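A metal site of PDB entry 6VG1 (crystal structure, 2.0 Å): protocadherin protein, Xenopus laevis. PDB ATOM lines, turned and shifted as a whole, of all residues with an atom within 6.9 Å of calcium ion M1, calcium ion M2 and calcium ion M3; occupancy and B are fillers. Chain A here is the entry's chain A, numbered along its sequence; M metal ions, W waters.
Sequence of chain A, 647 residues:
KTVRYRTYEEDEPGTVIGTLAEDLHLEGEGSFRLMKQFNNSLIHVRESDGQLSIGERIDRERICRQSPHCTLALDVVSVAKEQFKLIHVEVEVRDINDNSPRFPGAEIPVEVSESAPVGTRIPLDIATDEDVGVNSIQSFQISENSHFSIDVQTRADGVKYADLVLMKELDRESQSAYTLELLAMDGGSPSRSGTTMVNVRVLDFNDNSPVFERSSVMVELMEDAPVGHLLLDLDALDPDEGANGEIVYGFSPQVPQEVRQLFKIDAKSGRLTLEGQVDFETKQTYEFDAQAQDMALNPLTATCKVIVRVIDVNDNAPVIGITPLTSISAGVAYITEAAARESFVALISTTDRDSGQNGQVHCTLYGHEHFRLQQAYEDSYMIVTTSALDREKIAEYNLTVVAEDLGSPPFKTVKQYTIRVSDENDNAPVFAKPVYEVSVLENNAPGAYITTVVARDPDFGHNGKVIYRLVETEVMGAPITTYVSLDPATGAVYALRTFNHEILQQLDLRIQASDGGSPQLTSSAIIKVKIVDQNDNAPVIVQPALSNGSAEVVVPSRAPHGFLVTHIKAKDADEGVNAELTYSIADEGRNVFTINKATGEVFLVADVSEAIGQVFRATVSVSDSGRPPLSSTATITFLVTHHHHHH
Calcium ion M2 is bound by the side-chain carboxylate (OD2) of Asp 315 (2.1 Å), the side-chain carboxylate (OD1) of Asp 279 (2.2 Å), water W1 (2.3 Å), the side-chain carboxylate (OE1) of Glu 281 (2.4 Å), water W2 (2.4 Å) and the side-chain carboxylate (OE1) of Glu 223 (2.4 Å).
OE2 of Glu 281 is bound to calcium ion M1 (2.1 Å). Calcium ion M1 is bound by OD1 of Asp 312 (2.2 Å). OD1 of Asp 315 is bound to calcium ion M1. Calcium ion M1 is bound by the backbone carbonyl oxygen (O) of Val 313, at 2.3 Å. The side-chain carboxylate (OD1) of Asp 354 is bound to calcium ion M1 (2.3 Å). OE2 of Glu 223 is bound to calcium ion M1, at 2.3 Å. Calcium ion M1 has six donor atoms within binding distance. Slightly farther from calcium ion M1 lies the side-chain carboxylate (OE1) of Glu 281 (3.0 Å).
The backbone NH (N) of Gly 407 lies within hydrogen-bond range of the side-chain carboxylate (OD1) of Asp 405, at 3.1 Å. The side-chain carboxylate (OD1) of Asp 315 sits close to the side-chain amide nitrogen (ND2) of Asn 316 (3.2 Å). The side-chain carboxylate of Asp 312 sits at hydrogen-bond distance from the backbone NH of Ser 355. N of Glu 223 lies within hydrogen-bond range of O of Ile 311, at 3.1 Å. The side-chain carboxylate (OD1) of Asp 405 lies within hydrogen-bond range of the backbone NH (N) of Phe 411, at 2.9 Å. OG1 of Thr 282 sits at hydrogen-bond distance from OD2 of Asp 279, 2.8 Å away. OE1 of Glu 223 sits close to N of Phe 280.
Within 4 Å of calcium ion M3: Asn 314, Asn 316, Asp 352, Asp 354, Asn 358 and Asp 405.
Six residues have an atom within 4 Å of calcium ion M1: Glu 223, Glu 281, Asp 312, Val 313, Asp 315 and Asp 354. The nearest printed residue that does not touch calcium ion M1 is Asn 316 (4.2 Å).
Along chain A the residues within 4 Å of calcium ion M2 span positions 223 to 315. The nearest printed residue that does not touch calcium ion M2 is Phe 280 (4.2 Å).
Calcium ion M3 is bound by the backbone carbonyl oxygen (O) of Asn 358, the side-chain amide oxygen (OD1) of Asn 314, the side-chain carboxylate (OD1) of Asp 352, the side-chain carboxylate (OD2) of Asp 352, the side-chain carboxylate (OD2) of Asp 405, the backbone carbonyl oxygen (O) of Asn 316 and the side-chain carboxylate (OD2) of Asp 354.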
ATOM      1  N   GLU A 223     -37.470  35.582  19.657  1.00  0.00           N
ATOM      2  CA  GLU A 223     -36.912  35.527  18.310  1.00  0.00           C
ATOM      3  C   GLU A 223     -37.638  34.516  17.426  1.00  0.00           C
ATOM      4  O   GLU A 223     -37.410  34.495  16.207  1.00  0.00           O
ATOM      5  CB  GLU A 223     -35.412  35.208  18.326  1.00  0.00           C
ATOM      6  CG  GLU A 223     -34.990  33.841  18.742  1.00  0.00           C
ATOM      7  CD  GLU A 223     -33.527  33.543  18.389  1.00  0.00           C
ATOM      8  OE1 GLU A 223     -33.109  33.877  17.250  1.00  0.00           O
ATOM      9  OE2 GLU A 223     -32.784  33.002  19.245  1.00  0.00           O
ATOM     10  N   VAL A 278     -37.323  37.678  12.984  1.00  0.00           N
ATOM     11  CA  VAL A 278     -36.131  38.226  13.598  1.00  0.00           C
ATOM     12  C   VAL A 278     -35.224  37.064  13.987  1.00  0.00           C
ATOM     13  O   VAL A 278     -35.625  35.899  14.017  1.00  0.00           O
ATOM     14  CB  VAL A 278     -36.465  39.102  14.834  1.00  0.00           C
ATOM     15  CG1 VAL A 278     -37.230  40.336  14.426  1.00  0.00           C
ATOM     16  CG2 VAL A 278     -37.239  38.299  15.874  1.00  0.00           C
ATOM     17  N   ASP A 279     -33.959  37.383  14.280  1.00  0.00           N
ATOM     18  CA  ASP A 279     -32.984  36.359  14.633  1.00  0.00           C
ATOM     19  C   ASP A 279     -32.028  36.942  15.653  1.00  0.00           C
ATOM     20  O   ASP A 279     -31.179  37.777  15.319  1.00  0.00           O
ATOM     21  CB  ASP A 279     -32.225  35.884  13.393  1.00  0.00           C
ATOM     22  CG  ASP A 279     -31.161  34.888  13.727  1.00  0.00           C
ATOM     23  OD1 ASP A 279     -31.148  34.364  14.861  1.00  0.00           O
ATOM     24  OD2 ASP A 279     -30.311  34.612  12.840  1.00  0.00           O
ATOM     25  N   PHE A 280     -32.146  36.480  16.908  1.00  0.00           N
ATOM     26  CA  PHE A 280     -31.333  37.029  17.988  1.00  0.00           C
ATOM     27  C   PHE A 280     -29.854  36.933  17.658  1.00  0.00           C
ATOM     28  O   PHE A 280     -29.070  37.820  18.006  1.00  0.00           O
ATOM     29  CB  PHE A 280     -31.654  36.276  19.281  1.00  0.00           C
ATOM     30  CG  PHE A 280     -30.867  36.735  20.461  1.00  0.00           C
ATOM     31  CD1 PHE A 280     -31.380  37.683  21.314  1.00  0.00           C
ATOM     32  CD2 PHE A 280     -29.619  36.222  20.703  1.00  0.00           C
ATOM     33  CE1 PHE A 280     -30.659  38.115  22.403  1.00  0.00           C
ATOM     34  CE2 PHE A 280     -28.889  36.644  21.795  1.00  0.00           C
ATOM     35  CZ  PHE A 280     -29.412  37.593  22.651  1.00  0.00           C
ATOM     36  N   GLU A 281     -29.433  35.850  17.013  1.00  0.00           N
ATOM     37  CA  GLU A 281     -28.022  35.693  16.689  1.00  0.00           C
ATOM     38  C   GLU A 281     -27.537  36.656  15.622  1.00  0.00           C
ATOM     39  O   GLU A 281     -26.340  36.645  15.318  1.00  0.00           O
ATOM     40  CB  GLU A 281     -27.746  34.262  16.225  1.00  0.00           C
ATOM     41  CG  GLU A 281     -27.746  33.254  17.338  1.00  0.00           C
ATOM     42  CD  GLU A 281     -29.132  33.037  17.896  1.00  0.00           C
ATOM     43  OE1 GLU A 281     -30.120  33.059  17.106  1.00  0.00           O
ATOM     44  OE2 GLU A 281     -29.228  32.845  19.132  1.00  0.00           O
ATOM     45  N   THR A 282     -28.420  37.463  15.045  1.00  0.00           N
ATOM     46  CA  THR A 282     -28.067  38.398  13.991  1.00  0.00           C
ATOM     47  C   THR A 282     -28.228  39.841  14.434  1.00  0.00           C
ATOM     48  O   THR A 282     -27.347  40.673  14.211  1.00  0.00           O
ATOM     49  CB  THR A 282     -28.936  38.152  12.747  1.00  0.00           C
ATOM     50  OG1 THR A 282     -28.731  36.812  12.287  1.00  0.00           O
ATOM     51  CG2 THR A 282     -28.586  39.128  11.646  1.00  0.00           C
ATOM     52  N   ILE A 311     -35.372  38.338  22.248  1.00  0.00           N
ATOM     53  CA  ILE A 311     -35.009  37.393  23.299  1.00  0.00           C
ATOM     54  C   ILE A 311     -34.509  36.109  22.662  1.00  0.00           C
ATOM     55  O   ILE A 311     -35.122  35.596  21.721  1.00  0.00           O
ATOM     56  CB  ILE A 311     -36.192  37.113  24.238  1.00  0.00           C
ATOM     57  CG1 ILE A 311     -36.562  38.391  24.995  1.00  0.00           C
ATOM     58  CG2 ILE A 311     -35.847  35.979  25.172  1.00  0.00           C
ATOM     59  CD1 ILE A 311     -37.601  39.191  24.292  1.00  0.00           C
ATOM     60  N   ASP A 312     -33.437  35.556  23.217  1.00  0.00           N
ATOM     61  CA  ASP A 312     -32.763  34.424  22.599  1.00  0.00           C
ATOM     62  C   ASP A 312     -33.510  33.127  22.849  1.00  0.00           C
ATOM     63  O   ASP A 312     -34.005  32.880  23.946  1.00  0.00           O
ATOM     64  CB  ASP A 312     -31.342  34.313  23.149  1.00  0.00           C
ATOM     65  CG  ASP A 312     -30.590  33.120  22.595  1.00  0.00           C
ATOM     66  OD1 ASP A 312     -31.047  32.540  21.586  1.00  0.00           O
ATOM     67  OD2 ASP A 312     -29.535  32.763  23.179  1.00  0.00           O
ATOM     68  N   VAL A 313     -33.587  32.310  21.809  1.00  0.00           N
ATOM     69  CA  VAL A 313     -34.186  30.975  21.903  1.00  0.00           C
ATOM     70  C   VAL A 313     -33.121  29.945  21.574  1.00  0.00           C
ATOM     71  O   VAL A 313     -32.192  30.218  20.801  1.00  0.00           O
ATOM     72  CB  VAL A 313     -35.391  30.827  20.962  1.00  0.00           C
ATOM     73  CG1 VAL A 313     -35.909  29.399  21.011  1.00  0.00           C
ATOM     74  CG2 VAL A 313     -36.473  31.795  21.360  1.00  0.00           C
ATOM     75  N   ASN A 314     -33.249  28.758  22.153  1.00  0.00           N
ATOM     76  CA  ASN A 314     -32.286  27.687  21.880  1.00  0.00           C
ATOM     77  C   ASN A 314     -32.620  27.122  20.510  1.00  0.00           C
ATOM     78  O   ASN A 314     -33.248  26.066  20.366  1.00  0.00           O
ATOM     79  CB  ASN A 314     -32.295  26.616  22.947  1.00  0.00           C
ATOM     80  CG  ASN A 314     -31.058  25.747  22.881  1.00  0.00           C
ATOM     81  OD1 ASN A 314     -30.031  26.165  22.352  1.00  0.00           O
ATOM     82  ND2 ASN A 314     -31.147  24.539  23.431  1.00  0.00           N
ATOM     83  N   ASP A 315     -32.188  27.846  19.471  1.00  0.00           N
ATOM     84  CA  ASP A 315     -32.444  27.461  18.097  1.00  0.00           C
ATOM     85  C   ASP A 315     -31.157  27.090  17.356  1.00  0.00           C
ATOM     86  O   ASP A 315     -31.153  27.008  16.123  1.00  0.00           O
ATOM     87  CB  ASP A 315     -33.189  28.569  17.356  1.00  0.00           C
ATOM     88  CG  ASP A 315     -32.439  29.898  17.348  1.00  0.00           C
ATOM     89  OD1 ASP A 315     -31.551  30.122  18.200  1.00  0.00           O
ATOM     90  OD2 ASP A 315     -32.760  30.715  16.478  1.00  0.00           O
ATOM     91  N   ASN A 316     -30.084  26.830  18.098  1.00  0.00           N
ATOM     92  CA  ASN A 316     -28.851  26.331  17.507  1.00  0.00           C
ATOM     93  C   ASN A 316     -28.315  25.180  18.341  1.00  0.00           C
ATOM     94  O   ASN A 316     -28.427  25.184  19.568  1.00  0.00           O
ATOM     95  CB  ASN A 316     -27.768  27.418  17.417  1.00  0.00           C
ATOM     96  CG  ASN A 316     -28.064  28.446  16.338  1.00  0.00           C
ATOM     97  OD1 ASN A 316     -27.663  28.282  15.175  1.00  0.00           O
ATOM     98  ND2 ASN A 316     -28.778  29.490  16.714  1.00  0.00           N
ATOM     99  N   ALA A 317     -27.711  24.210  17.672  1.00  0.00           N
ATOM    100  CA  ALA A 317     -27.054  23.103  18.327  1.00  0.00           C
ATOM    101  C   ALA A 317     -25.557  23.306  18.311  1.00  0.00           C
ATOM    102  O   ALA A 317     -25.046  24.134  17.561  1.00  0.00           O
ATOM    103  CB  ALA A 317     -27.404  21.784  17.642  1.00  0.00           C
ATOM    104  N   PRO A 318     -24.821  22.581  19.154  1.00  0.00           N
ATOM    105  CA  PRO A 318     -23.357  22.688  19.110  1.00  0.00           C
ATOM    106  C   PRO A 318     -22.776  22.251  17.778  1.00  0.00           C
ATOM    107  O   PRO A 318     -23.272  21.321  17.129  1.00  0.00           O
ATOM    108  CB  PRO A 318     -22.900  21.763  20.243  1.00  0.00           C
ATOM    109  CG  PRO A 318     -24.061  21.790  21.204  1.00  0.00           C
ATOM    110  CD  PRO A 318     -25.308  21.878  20.354  1.00  0.00           C
ATOM    111  N   ASP A 352     -21.643  27.104  20.128  1.00  0.00           N
ATOM    112  CA  ASP A 352     -23.105  27.189  20.083  1.00  0.00           C
ATOM    113  C   ASP A 352     -23.453  28.639  19.809  1.00  0.00           C
ATOM    114  O   ASP A 352     -23.065  29.520  20.573  1.00  0.00           O
ATOM    115  CB  ASP A 352     -23.743  26.723  21.398  1.00  0.00           C
ATOM    116  CG  ASP A 352     -25.247  26.445  21.275  1.00  0.00           C
ATOM    117  OD1 ASP A 352     -25.655  25.277  21.471  1.00  0.00           O
ATOM    118  OD2 ASP A 352     -26.032  27.396  21.017  1.00  0.00           O
ATOM    119  N   ARG A 353     -24.179  28.900  18.713  1.00  0.00           N
ATOM    120  CA  ARG A 353     -24.457  30.273  18.305  1.00  0.00           C
ATOM    121  C   ARG A 353     -25.303  31.024  19.334  1.00  0.00           C
ATOM    122  O   ARG A 353     -25.321  32.262  19.311  1.00  0.00           O
ATOM    123  CB  ARG A 353     -25.233  30.319  16.972  1.00  0.00           C
ATOM    124  CG  ARG A 353     -24.564  29.631  15.798  1.00  0.00           C
ATOM    125  CD  ARG A 353     -23.568  30.572  15.138  1.00  0.00           C
ATOM    126  NE  ARG A 353     -24.218  31.745  14.553  1.00  0.00           N
ATOM    127  CZ  ARG A 353     -23.556  32.789  14.093  1.00  0.00           C
ATOM    128  NH1 ARG A 353     -22.231  32.802  14.166  1.00  0.00           N
ATOM    129  NH2 ARG A 353     -24.201  33.826  13.573  1.00  0.00           N
ATOM    130  N   ASP A 354     -26.061  30.313  20.163  1.00  0.00           N
ATOM    131  CA  ASP A 354     -26.958  30.990  21.084  1.00  0.00           C
ATOM    132  C   ASP A 354     -26.164  31.647  22.221  1.00  0.00           C
ATOM    133  O   ASP A 354     -24.931  31.635  22.262  1.00  0.00           O
ATOM    134  CB  ASP A 354     -27.973  30.010  21.677  1.00  0.00           C
ATOM    135  CG  ASP A 354     -28.753  29.280  20.614  1.00  0.00           C
ATOM    136  OD1 ASP A 354     -29.334  29.951  19.722  1.00  0.00           O
ATOM    137  OD2 ASP A 354     -28.793  28.032  20.669  1.00  0.00           O
ATOM    138  N   SER A 355     -26.900  32.195  23.183  1.00  0.00           N
ATOM    139  CA  SER A 355     -26.338  32.884  24.342  1.00  0.00           C
ATOM    140  C   SER A 355     -26.888  32.288  25.632  1.00  0.00           C
ATOM    141  O   SER A 355     -27.866  31.532  25.642  1.00  0.00           O
ATOM    142  CB  SER A 355     -26.652  34.383  24.286  1.00  0.00           C
ATOM    143  OG  SER A 355     -26.032  34.973  23.167  1.00  0.00           O
ATOM    144  N   GLN A 357     -27.134  29.926  28.978  1.00  0.00           N
ATOM    145  CA  GLN A 357     -27.067  28.468  29.070  1.00  0.00           C
ATOM    146  C   GLN A 357     -27.299  27.813  27.720  1.00  0.00           C
ATOM    147  O   GLN A 357     -26.713  26.761  27.430  1.00  0.00           O
ATOM    148  CB  GLN A 357     -28.109  27.964  30.066  1.00  0.00           C
ATOM    149  CG  GLN A 357     -27.913  28.425  31.497  1.00  0.00           C
ATOM    150  CD  GLN A 357     -26.993  27.523  32.287  1.00  0.00           C
ATOM    151  OE1 GLN A 357     -27.132  26.298  32.273  1.00  0.00           O
ATOM    152  NE2 GLN A 357     -26.025  28.120  32.971  1.00  0.00           N
ATOM    153  N   ASN A 358     -28.149  28.413  26.890  1.00  0.00           N
ATOM    154  CA  ASN A 358     -28.456  27.822  25.597  1.00  0.00           C
ATOM    155  C   ASN A 358     -27.226  27.783  24.700  1.00  0.00           C
ATOM    156  O   ASN A 358     -27.185  26.957  23.775  1.00  0.00           O
ATOM    157  CB  ASN A 358     -29.583  28.594  24.913  1.00  0.00           C
ATOM    158  CG  ASN A 358     -30.892  28.492  25.668  1.00  0.00           C
ATOM    159  OD1 ASN A 358     -31.149  27.513  26.357  1.00  0.00           O
ATOM    160  ND2 ASN A 358     -31.749  29.487  25.491  1.00  0.00           N
ATOM    161  N   GLY A 359     -26.221  28.624  24.964  1.00  0.00           N
ATOM    162  CA  GLY A 359     -25.019  28.657  24.161  1.00  0.00           C
ATOM    163  C   GLY A 359     -23.790  28.090  24.827  1.00  0.00           C
ATOM    164  O   GLY A 359     -22.698  28.204  24.274  1.00  0.00           O
ATOM    165  N   GLN A 360     -23.926  27.485  26.000  1.00  0.00           N
ATOM    166  CA  GLN A 360     -22.804  26.997  26.780  1.00  0.00           C
ATOM    167  C   GLN A 360     -22.661  25.511  26.533  1.00  0.00           C
ATOM    168  O   GLN A 360     -23.632  24.755  26.676  1.00  0.00           O
ATOM    169  CB  GLN A 360     -23.060  27.284  28.254  1.00  0.00           C
ATOM    170  CG  GLN A 360     -21.866  27.178  29.126  1.00  0.00           C
ATOM    171  CD  GLN A 360     -22.111  27.887  30.446  1.00  0.00           C
ATOM    172  OE1 GLN A 360     -22.545  29.036  30.474  1.00  0.00           O
ATOM    173  NE2 GLN A 360     -21.838  27.203  31.545  1.00  0.00           N
ATOM    174  N   VAL A 361     -21.451  25.076  26.174  1.00  0.00           N
ATOM    175  CA  VAL A 361     -21.228  23.723  25.677  1.00  0.00           C
ATOM    176  C   VAL A 361     -20.368  22.924  26.644  1.00  0.00           C
ATOM    177  O   VAL A 361     -19.365  23.422  27.172  1.00  0.00           O
ATOM    178  CB  VAL A 361     -20.571  23.729  24.287  1.00  0.00           C
ATOM    179  CG1 VAL A 361     -21.432  24.466  23.295  1.00  0.00           C
ATOM    180  CG2 VAL A 361     -19.171  24.362  24.361  1.00  0.00           C
ATOM    181  N   ASP A 405     -25.302  21.439  24.795  1.00  0.00           N
ATOM    182  CA  ASP A 405     -25.507  22.761  25.377  1.00  0.00           C
ATOM    183  C   ASP A 405     -26.321  22.599  26.667  1.00  0.00           C
ATOM    184  O   ASP A 405     -26.738  21.489  27.032  1.00  0.00           O
ATOM    185  CB  ASP A 405     -26.163  23.730  24.368  1.00  0.00           C
ATOM    186  CG  ASP A 405     -27.632  23.473  24.130  1.00  0.00           C
ATOM    187  OD1 ASP A 405     -28.233  22.629  24.843  1.00  0.00           O
ATOM    188  OD2 ASP A 405     -28.186  24.119  23.203  1.00  0.00           O
ATOM    189  N   LEU A 406     -26.546  23.704  27.373  1.00  0.00           N
ATOM    190  CA  LEU A 406     -27.245  23.667  28.650  1.00  0.00           C
ATOM    191  C   LEU A 406     -28.669  24.196  28.527  1.00  0.00           C
ATOM    192  O   LEU A 406     -29.230  24.702  29.498  1.00  0.00           O
ATOM    193  CB  LEU A 406     -26.468  24.437  29.703  1.00  0.00           C
ATOM    194  CG  LEU A 406     -25.368  23.681  30.427  1.00  0.00           C
ATOM    195  CD1 LEU A 406     -25.986  22.616  31.351  1.00  0.00           C
ATOM    196  CD2 LEU A 406     -24.370  23.005  29.484  1.00  0.00           C
ATOM    197  N   GLY A 407     -29.276  24.048  27.357  1.00  0.00           N
ATOM    198  CA  GLY A 407     -30.673  24.387  27.196  1.00  0.00           C
ATOM    199  C   GLY A 407     -31.572  23.389  27.909  1.00  0.00           C
ATOM    200  O   GLY A 407     -31.153  22.377  28.440  1.00  0.00           O
ATOM    201  N   PHE A 411     -29.551  20.557  23.280  1.00  0.00           N
ATOM    202  CA  PHE A 411     -29.124  20.018  21.990  1.00  0.00           C
ATOM    203  C   PHE A 411     -27.866  19.204  22.205  1.00  0.00           C
ATOM    204  O   PHE A 411     -26.980  19.607  22.965  1.00  0.00           O
ATOM    205  CB  PHE A 411     -28.848  21.141  20.985  1.00  0.00           C
ATOM    206  CG  PHE A 411     -30.058  21.555  20.151  1.00  0.00           C
ATOM    207  CD1 PHE A 411     -30.546  20.708  19.163  1.00  0.00           C
ATOM    208  CD2 PHE A 411     -30.678  22.788  20.349  1.00  0.00           C
ATOM    209  CE1 PHE A 411     -31.648  21.087  18.401  1.00  0.00           C
ATOM    210  CE2 PHE A 411     -31.760  23.150  19.600  1.00  0.00           C
ATOM    211  CZ  PHE A 411     -32.253  22.319  18.618  1.00  0.00           C
HETATM  212 CA    CA M   1     -30.907  31.669  19.613  1.00  0.00          CA
HETATM  213 CA    CA M   2     -31.915  32.430  15.716  1.00  0.00          CA
HETATM  214 CA    CA M   3     -27.821  26.060  21.777  1.00  0.00          CA
HETATM  215  O   HOH W   1     -30.516  31.076  14.471  1.00  0.00           O
HETATM  216  O   HOH W   2     -33.341  32.554  13.782  1.00  0.00           O
